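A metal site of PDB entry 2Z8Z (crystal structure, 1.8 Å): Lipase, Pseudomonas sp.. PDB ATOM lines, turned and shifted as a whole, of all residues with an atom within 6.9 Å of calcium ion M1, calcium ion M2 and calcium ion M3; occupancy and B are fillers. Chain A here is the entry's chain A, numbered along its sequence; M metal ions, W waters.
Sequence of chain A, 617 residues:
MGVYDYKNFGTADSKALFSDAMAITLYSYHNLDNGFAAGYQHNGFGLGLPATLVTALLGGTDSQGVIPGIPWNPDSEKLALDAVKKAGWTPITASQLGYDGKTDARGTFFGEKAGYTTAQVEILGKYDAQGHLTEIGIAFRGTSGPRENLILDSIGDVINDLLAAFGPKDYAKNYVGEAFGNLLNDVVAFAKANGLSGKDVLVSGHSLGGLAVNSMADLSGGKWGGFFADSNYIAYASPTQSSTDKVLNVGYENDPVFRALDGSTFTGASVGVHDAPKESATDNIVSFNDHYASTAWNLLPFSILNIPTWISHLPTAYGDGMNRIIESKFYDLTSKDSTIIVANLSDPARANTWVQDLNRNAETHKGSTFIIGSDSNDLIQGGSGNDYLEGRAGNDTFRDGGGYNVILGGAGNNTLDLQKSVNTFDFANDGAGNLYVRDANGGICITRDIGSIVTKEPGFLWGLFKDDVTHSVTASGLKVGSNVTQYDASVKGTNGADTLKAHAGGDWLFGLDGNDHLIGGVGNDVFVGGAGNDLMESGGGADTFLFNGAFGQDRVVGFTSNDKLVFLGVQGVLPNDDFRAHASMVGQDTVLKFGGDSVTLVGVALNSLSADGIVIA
The side-chain amide nitrogen (ND2) of Asn 495 lies close to the backbone NH (N) of Asp 513 (3.1 Å). The backbone carbonyl oxygen (O) of Val 528 lies within hydrogen-bond range of the backbone NH (N) of Gly 511 (3.0 Å). OG1 of Thr 494 lies within hydrogen-bond range of N of Gly 496 (3.1 Å). O of Ser 598 sits at hydrogen-bond distance from N of Asp 554, at 2.9 Å.
Seven residues have an atom within 4 Å of calcium ion M1: Thr 494, Gly 496, Asp 498, Gly 511, Leu 512, Asp 513 and Asp 516.
Eight residues have an atom within 4 Å of calcium ion M2: Leu 512, Asp 513, Gly 514, Asp 516, Gly 529, Gly 530, Ala 531 and Asp 534.
Six residues have an atom within 4 Å of calcium ion M3: Gly 530, Ala 531, Gly 532, Asp 534, Phe 551 and Asp 554.
Calcium ion M1 is bound by O of Gly 511, O of Thr 494, O of Gly 496, O of Asp 513, OD2 of Asp 498, OD1 of Asp 516 and OD2 of Asp 516.
Calcium ion M2 is bound by the backbone carbonyl oxygen of Leu 512, the backbone carbonyl oxygen of Gly 514, the backbone carbonyl oxygen of Ala 531, the side-chain carboxylate of Asp 534, the backbone carbonyl oxygen of Gly 529 and the side-chain carboxylate of Asp 516. Calcium ion M2 has six donor atoms within binding distance. Slightly farther from calcium ion M2 lies the side-chain carboxylate (OD2) of Asp 534 (3.0 Å).
Calcium ion M3 is bound by O of Phe 551 (2.2 Å), O of Gly 530 (2.2 Å), O of Gly 532 (2.3 Å), OD2 of Asp 534 (2.3 Å), OD1 of Asp 554 (2.4 Å) and water W1 (2.4 Å). Slightly farther from calcium ion M3 lies the side-chain carboxylate (OD2) of Asp 554 (3.1 Å).
Water W1 lies within hydrogen-bond range of OD2 of Asp 554 (2.6 Å) and N of Gly 530 (3.4 Å).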
ATOM      1  N   GLY A 493     -23.065  13.514  14.581  1.00  0.00           N
ATOM      2  CA  GLY A 493     -24.205  14.030  15.317  1.00  0.00           C
ATOM      3  C   GLY A 493     -25.039  12.979  16.057  1.00  0.00           C
ATOM      4  O   GLY A 493     -24.527  11.956  16.519  1.00  0.00           O
ATOM      5  N   THR A 494     -26.314  13.232  16.126  1.00  0.00           N
ATOM      6  CA  THR A 494     -27.297  12.388  16.761  1.00  0.00           C
ATOM      7  C   THR A 494     -28.511  12.297  15.858  1.00  0.00           C
ATOM      8  O   THR A 494     -28.543  12.958  14.831  1.00  0.00           O
ATOM      9  CB  THR A 494     -27.710  12.998  18.102  1.00  0.00           C
ATOM     10  OG1 THR A 494     -28.554  14.133  17.909  1.00  0.00           O
ATOM     11  CG2 THR A 494     -26.504  13.333  18.961  1.00  0.00           C
ATOM     12  N   ASN A 495     -29.503  11.502  16.243  1.00  0.00           N
ATOM     13  CA  ASN A 495     -30.749  11.435  15.464  1.00  0.00           C
ATOM     14  C   ASN A 495     -31.721  12.606  15.722  1.00  0.00           C
ATOM     15  O   ASN A 495     -32.798  12.621  15.195  1.00  0.00           O
ATOM     16  CB  ASN A 495     -31.421  10.074  15.650  1.00  0.00           C
ATOM     17  CG  ASN A 495     -30.709   8.980  14.878  1.00  0.00           C
ATOM     18  OD1 ASN A 495     -30.669   7.831  15.329  1.00  0.00           O
ATOM     19  ND2 ASN A 495     -30.145   9.321  13.728  1.00  0.00           N
ATOM     20  N   GLY A 496     -31.313  13.589  16.542  1.00  0.00           N
ATOM     21  CA  GLY A 496     -32.023  14.860  16.679  1.00  0.00           C
ATOM     22  C   GLY A 496     -31.291  15.958  15.879  1.00  0.00           C
ATOM     23  O   GLY A 496     -30.349  15.665  15.146  1.00  0.00           O
ATOM     24  N   ALA A 497     -31.740  17.178  16.037  1.00  0.00           N
ATOM     25  CA  ALA A 497     -31.146  18.363  15.378  1.00  0.00           C
ATOM     26  C   ALA A 497     -29.810  18.749  16.063  1.00  0.00           C
ATOM     27  O   ALA A 497     -29.779  18.988  17.286  1.00  0.00           O
ATOM     28  CB  ALA A 497     -32.109  19.485  15.473  1.00  0.00           C
ATOM     29  N   ASP A 498     -28.725  18.717  15.294  1.00  0.00           N
ATOM     30  CA  ASP A 498     -27.404  18.998  15.788  1.00  0.00           C
ATOM     31  C   ASP A 498     -26.796  20.150  14.990  1.00  0.00           C
ATOM     32  O   ASP A 498     -27.071  20.312  13.840  1.00  0.00           O
ATOM     33  CB  ASP A 498     -26.466  17.841  15.548  1.00  0.00           C
ATOM     34  CG  ASP A 498     -27.035  16.483  15.958  1.00  0.00           C
ATOM     35  OD1 ASP A 498     -27.285  16.260  17.163  1.00  0.00           O
ATOM     36  OD2 ASP A 498     -27.190  15.598  15.076  1.00  0.00           O
ATOM     37  N   LEU A 500     -22.977  20.723  13.878  1.00  0.00           N
ATOM     38  CA  LEU A 500     -21.673  20.136  13.858  1.00  0.00           C
ATOM     39  C   LEU A 500     -20.735  21.090  13.115  1.00  0.00           C
ATOM     40  O   LEU A 500     -21.075  21.596  12.067  1.00  0.00           O
ATOM     41  CB  LEU A 500     -21.661  18.813  13.120  1.00  0.00           C
ATOM     42  CG  LEU A 500     -22.724  17.775  13.473  1.00  0.00           C
ATOM     43  CD1 LEU A 500     -22.488  16.594  12.595  1.00  0.00           C
ATOM     44  CD2 LEU A 500     -22.683  17.411  15.008  1.00  0.00           C
ATOM     45  N   PHE A 510     -21.293  13.932   9.777  1.00  0.00           N
ATOM     46  CA  PHE A 510     -22.434  12.978   9.742  1.00  0.00           C
ATOM     47  C   PHE A 510     -23.598  13.495  10.619  1.00  0.00           C
ATOM     48  O   PHE A 510     -23.604  13.329  11.866  1.00  0.00           O
ATOM     49  CB  PHE A 510     -21.944  11.617  10.254  1.00  0.00           C
ATOM     50  CG  PHE A 510     -20.901  10.967   9.392  1.00  0.00           C
ATOM     51  CD1 PHE A 510     -21.177  10.590   8.078  1.00  0.00           C
ATOM     52  CD2 PHE A 510     -19.609  10.696   9.881  1.00  0.00           C
ATOM     53  CE1 PHE A 510     -20.240   9.970   7.297  1.00  0.00           C
ATOM     54  CE2 PHE A 510     -18.654  10.065   9.059  1.00  0.00           C
ATOM     55  CZ  PHE A 510     -18.977   9.698   7.781  1.00  0.00           C
ATOM     56  N   GLY A 511     -24.555  14.175  10.012  1.00  0.00           N
ATOM     57  CA  GLY A 511     -25.673  14.706  10.734  1.00  0.00           C
ATOM     58  C   GLY A 511     -26.625  13.647  11.277  1.00  0.00           C
ATOM     59  O   GLY A 511     -27.322  13.895  12.300  1.00  0.00           O
ATOM     60  N   LEU A 512     -26.684  12.507  10.576  1.00  0.00           N
ATOM     61  CA  LEU A 512     -27.694  11.467  10.855  1.00  0.00           C
ATOM     62  C   LEU A 512     -29.122  12.089  10.820  1.00  0.00           C
ATOM     63  O   LEU A 512     -29.375  13.097  10.098  1.00  0.00           O
ATOM     64  CB  LEU A 512     -27.403  10.836  12.210  1.00  0.00           C
ATOM     65  CG  LEU A 512     -25.974  10.376  12.454  1.00  0.00           C
ATOM     66  CD1 LEU A 512     -25.810   9.856  13.884  1.00  0.00           C
ATOM     67  CD2 LEU A 512     -25.513   9.371  11.422  1.00  0.00           C
ATOM     68  N   ASP A 513     -30.089  11.469  11.514  1.00  0.00           N
ATOM     69  CA  ASP A 513     -31.442  11.944  11.420  1.00  0.00           C
ATOM     70  C   ASP A 513     -31.626  13.324  12.028  1.00  0.00           C
ATOM     71  O   ASP A 513     -30.771  13.803  12.786  1.00  0.00           O
ATOM     72  CB  ASP A 513     -32.445  10.974  12.067  1.00  0.00           C
ATOM     73  CG  ASP A 513     -32.417   9.550  11.486  1.00  0.00           C
ATOM     74  OD1 ASP A 513     -31.749   9.281  10.454  1.00  0.00           O
ATOM     75  OD2 ASP A 513     -33.121   8.706  12.094  1.00  0.00           O
ATOM     76  N   GLY A 514     -32.745  13.977  11.668  1.00  0.00           N
ATOM     77  CA  GLY A 514     -33.130  15.257  12.160  1.00  0.00           C
ATOM     78  C   GLY A 514     -32.555  16.365  11.264  1.00  0.00           C
ATOM     79  O   GLY A 514     -31.710  16.086  10.384  1.00  0.00           O
ATOM     80  N   ASN A 515     -33.020  17.597  11.515  1.00  0.00           N
ATOM     81  CA  ASN A 515     -32.658  18.773  10.733  1.00  0.00           C
ATOM     82  C   ASN A 515     -31.394  19.378  11.275  1.00  0.00           C
ATOM     83  O   ASN A 515     -31.409  20.063  12.294  1.00  0.00           O
ATOM     84  CB  ASN A 515     -33.798  19.770  10.689  1.00  0.00           C
ATOM     85  CG  ASN A 515     -35.107  19.180  10.164  1.00  0.00           C
ATOM     86  OD1 ASN A 515     -35.137  18.132   9.517  1.00  0.00           O
ATOM     87  ND2 ASN A 515     -36.181  19.821  10.492  1.00  0.00           N
ATOM     88  N   ASP A 516     -30.290  19.102  10.604  1.00  0.00           N
ATOM     89  CA  ASP A 516     -28.949  19.458  11.086  1.00  0.00           C
ATOM     90  C   ASP A 516     -28.350  20.690  10.396  1.00  0.00           C
ATOM     91  O   ASP A 516     -28.823  21.124   9.363  1.00  0.00           O
ATOM     92  CB  ASP A 516     -28.039  18.268  10.958  1.00  0.00           C
ATOM     93  CG  ASP A 516     -28.597  17.046  11.709  1.00  0.00           C
ATOM     94  OD1 ASP A 516     -28.901  17.194  12.941  1.00  0.00           O
ATOM     95  OD2 ASP A 516     -28.699  15.984  11.068  1.00  0.00           O
ATOM     96  N   LEU A 518     -24.775  21.914   9.441  1.00  0.00           N
ATOM     97  CA  LEU A 518     -23.441  21.437   9.232  1.00  0.00           C
ATOM     98  C   LEU A 518     -22.509  22.534   8.745  1.00  0.00           C
ATOM     99  O   LEU A 518     -22.676  23.020   7.638  1.00  0.00           O
ATOM    100  CB  LEU A 518     -23.441  20.296   8.240  1.00  0.00           C
ATOM    101  CG  LEU A 518     -23.674  18.909   8.834  1.00  0.00           C
ATOM    102  CD1 LEU A 518     -24.601  18.802   9.941  1.00  0.00           C
ATOM    103  CD2 LEU A 518     -23.907  17.843   7.767  1.00  0.00           C
ATOM    104  N   VAL A 528     -22.476  14.714   4.995  1.00  0.00           N
ATOM    105  CA  VAL A 528     -23.576  13.743   4.901  1.00  0.00           C
ATOM    106  C   VAL A 528     -24.708  14.147   5.842  1.00  0.00           C
ATOM    107  O   VAL A 528     -24.784  13.760   7.053  1.00  0.00           O
ATOM    108  CB  VAL A 528     -23.110  12.309   5.208  1.00  0.00           C
ATOM    109  CG1 VAL A 528     -24.232  11.322   4.828  1.00  0.00           C
ATOM    110  CG2 VAL A 528     -21.802  11.954   4.481  1.00  0.00           C
ATOM    111  N   GLY A 529     -25.610  14.978   5.317  1.00  0.00           N
ATOM    112  CA  GLY A 529     -26.714  15.501   6.133  1.00  0.00           C
ATOM    113  C   GLY A 529     -27.562  14.387   6.724  1.00  0.00           C
ATOM    114  O   GLY A 529     -28.105  14.508   7.818  1.00  0.00           O
ATOM    115  N   GLY A 530     -27.686  13.302   5.981  1.00  0.00           N
ATOM    116  CA  GLY A 530     -28.641  12.226   6.303  1.00  0.00           C
ATOM    117  C   GLY A 530     -30.109  12.601   6.117  1.00  0.00           C
ATOM    118  O   GLY A 530     -30.491  13.604   5.435  1.00  0.00           O
ATOM    119  N   ALA A 531     -30.953  11.813   6.766  1.00  0.00           N
ATOM    120  CA  ALA A 531     -32.373  12.127   6.845  1.00  0.00           C
ATOM    121  C   ALA A 531     -32.582  13.448   7.488  1.00  0.00           C
ATOM    122  O   ALA A 531     -31.679  13.928   8.203  1.00  0.00           O
ATOM    123  CB  ALA A 531     -33.106  11.050   7.648  1.00  0.00           C
ATOM    124  N   GLY A 532     -33.727  14.050   7.227  1.00  0.00           N
ATOM    125  CA  GLY A 532     -34.012  15.377   7.662  1.00  0.00           C
ATOM    126  C   GLY A 532     -33.573  16.455   6.676  1.00  0.00           C
ATOM    127  O   GLY A 532     -32.915  16.174   5.702  1.00  0.00           O
ATOM    128  N   ASN A 533     -33.872  17.686   7.027  1.00  0.00           N
ATOM    129  CA  ASN A 533     -33.689  18.879   6.156  1.00  0.00           C
ATOM    130  C   ASN A 533     -32.499  19.579   6.768  1.00  0.00           C
ATOM    131  O   ASN A 533     -32.589  20.213   7.816  1.00  0.00           O
ATOM    132  CB  ASN A 533     -34.963  19.731   6.143  1.00  0.00           C
ATOM    133  CG  ASN A 533     -36.201  18.900   5.714  1.00  0.00           C
ATOM    134  OD1 ASN A 533     -36.099  17.893   5.056  1.00  0.00           O
ATOM    135  ND2 ASN A 533     -37.381  19.384   6.085  1.00  0.00           N
ATOM    136  N   ASP A 534     -31.372  19.369   6.134  1.00  0.00           N
ATOM    137  CA  ASP A 534     -30.120  19.783   6.655  1.00  0.00           C
ATOM    138  C   ASP A 534     -29.634  21.040   5.962  1.00  0.00           C
ATOM    139  O   ASP A 534     -29.742  21.124   4.741  1.00  0.00           O
ATOM    140  CB  ASP A 534     -29.139  18.692   6.508  1.00  0.00           C
ATOM    141  CG  ASP A 534     -29.591  17.421   7.183  1.00  0.00           C
ATOM    142  OD1 ASP A 534     -29.761  17.400   8.424  1.00  0.00           O
ATOM    143  OD2 ASP A 534     -29.823  16.459   6.459  1.00  0.00           O
ATOM    144  N   MET A 536     -26.254  23.019   5.111  1.00  0.00           N
ATOM    145  CA  MET A 536     -24.887  22.617   4.995  1.00  0.00           C
ATOM    146  C   MET A 536     -24.040  23.658   4.358  1.00  0.00           C
ATOM    147  O   MET A 536     -24.315  24.069   3.239  1.00  0.00           O
ATOM    148  CB  MET A 536     -24.778  21.284   4.281  1.00  0.00           C
ATOM    149  CG  MET A 536     -25.642  20.194   4.905  1.00  0.00           C
ATOM    150  SD  MET A 536     -25.463  18.625   4.112  1.00  0.00           S
ATOM    151  CE  MET A 536     -26.639  18.774   2.831  1.00  0.00           C
ATOM    152  N   PHE A 547     -25.654  12.569  -0.870  1.00  0.00           N
ATOM    153  CA  PHE A 547     -27.090  12.426  -0.703  1.00  0.00           C
ATOM    154  C   PHE A 547     -27.470  11.002  -1.093  1.00  0.00           C
ATOM    155  O   PHE A 547     -27.126  10.572  -2.170  1.00  0.00           O
ATOM    156  CB  PHE A 547     -27.836  13.416  -1.573  1.00  0.00           C
ATOM    157  CG  PHE A 547     -27.383  14.830  -1.370  1.00  0.00           C
ATOM    158  CD1 PHE A 547     -27.933  15.603  -0.379  1.00  0.00           C
ATOM    159  CD2 PHE A 547     -26.430  15.387  -2.214  1.00  0.00           C
ATOM    160  CE1 PHE A 547     -27.486  16.939  -0.194  1.00  0.00           C
ATOM    161  CE2 PHE A 547     -25.970  16.662  -1.977  1.00  0.00           C
ATOM    162  CZ  PHE A 547     -26.516  17.439  -1.005  1.00  0.00           C
ATOM    163  N   ALA A 550     -33.858   8.671   1.267  1.00  0.00           N
ATOM    164  CA  ALA A 550     -34.889   9.720   1.355  1.00  0.00           C
ATOM    165  C   ALA A 550     -34.244  10.857   2.133  1.00  0.00           C
ATOM    166  O   ALA A 550     -34.396  10.991   3.367  1.00  0.00           O
ATOM    167  CB  ALA A 550     -36.121   9.220   2.041  1.00  0.00           C
ATOM    168  N   PHE A 551     -33.461  11.643   1.422  1.00  0.00           N
ATOM    169  CA  PHE A 551     -32.475  12.527   2.079  1.00  0.00           C
ATOM    170  C   PHE A 551     -33.037  13.866   2.533  1.00  0.00           C
ATOM    171  O   PHE A 551     -32.364  14.651   3.190  1.00  0.00           O
ATOM    172  CB  PHE A 551     -31.247  12.684   1.218  1.00  0.00           C
ATOM    173  CG  PHE A 551     -31.492  13.363  -0.109  1.00  0.00           C
ATOM    174  CD1 PHE A 551     -31.559  14.733  -0.188  1.00  0.00           C
ATOM    175  CD2 PHE A 551     -31.594  12.616  -1.264  1.00  0.00           C
ATOM    176  CE1 PHE A 551     -31.791  15.382  -1.467  1.00  0.00           C
ATOM    177  CE2 PHE A 551     -31.785  13.216  -2.485  1.00  0.00           C
ATOM    178  CZ  PHE A 551     -31.907  14.600  -2.601  1.00  0.00           C
ATOM    179  N   GLY A 552     -34.307  14.115   2.209  1.00  0.00           N
ATOM    180  CA  GLY A 552     -34.989  15.324   2.668  1.00  0.00           C
ATOM    181  C   GLY A 552     -34.827  16.547   1.800  1.00  0.00           C
ATOM    182  O   GLY A 552     -34.584  16.428   0.564  1.00  0.00           O
ATOM    183  N   GLN A 553     -35.097  17.708   2.410  1.00  0.00           N
ATOM    184  CA  GLN A 553     -35.077  19.011   1.712  1.00  0.00           C
ATOM    185  C   GLN A 553     -33.878  19.743   2.321  1.00  0.00           C
ATOM    186  O   GLN A 553     -33.976  20.336   3.421  1.00  0.00           O
ATOM    187  CB  GLN A 553     -36.341  19.837   1.881  1.00  0.00           C
ATOM    188  CG  GLN A 553     -37.620  19.023   1.925  1.00  0.00           C
ATOM    189  CD  GLN A 553     -37.786  18.177   0.739  1.00  0.00           C
ATOM    190  OE1 GLN A 553     -38.155  17.002   0.848  1.00  0.00           O
ATOM    191  NE2 GLN A 553     -37.542  18.735  -0.409  1.00  0.00           N
ATOM    192  N   ASP A 554     -32.770  19.681   1.602  1.00  0.00           N
ATOM    193  CA  ASP A 554     -31.507  20.224   2.099  1.00  0.00           C
ATOM    194  C   ASP A 554     -31.199  21.567   1.436  1.00  0.00           C
ATOM    195  O   ASP A 554     -31.678  21.819   0.343  1.00  0.00           O
ATOM    196  CB  ASP A 554     -30.363  19.260   1.819  1.00  0.00           C
ATOM    197  CG  ASP A 554     -30.478  17.925   2.547  1.00  0.00           C
ATOM    198  OD1 ASP A 554     -31.059  17.846   3.707  1.00  0.00           O
ATOM    199  OD2 ASP A 554     -29.921  16.960   1.953  1.00  0.00           O
ATOM    200  N   SER A 598     -34.926  17.020  -2.153  1.00  0.00           N
ATOM    201  CA  SER A 598     -34.427  18.168  -2.908  1.00  0.00           C
ATOM    202  C   SER A 598     -33.193  18.747  -2.242  1.00  0.00           C
ATOM    203  O   SER A 598     -32.988  18.600  -1.039  1.00  0.00           O
ATOM    204  CB  SER A 598     -35.491  19.239  -3.048  1.00  0.00           C
ATOM    205  OG  SER A 598     -35.699  19.971  -1.854  1.00  0.00           O
HETATM  206 CA    CA M   1     -28.833  14.882  13.548  1.00  0.00          CA
HETATM  207 CA    CA M   2     -29.943  15.157   9.180  1.00  0.00          CA
HETATM  208 CA    CA M   3     -30.935  15.619   4.569  1.00  0.00          CA
HETATM  209  O   HOH W   1     -28.872  15.114   3.419  1.00  0.00           O
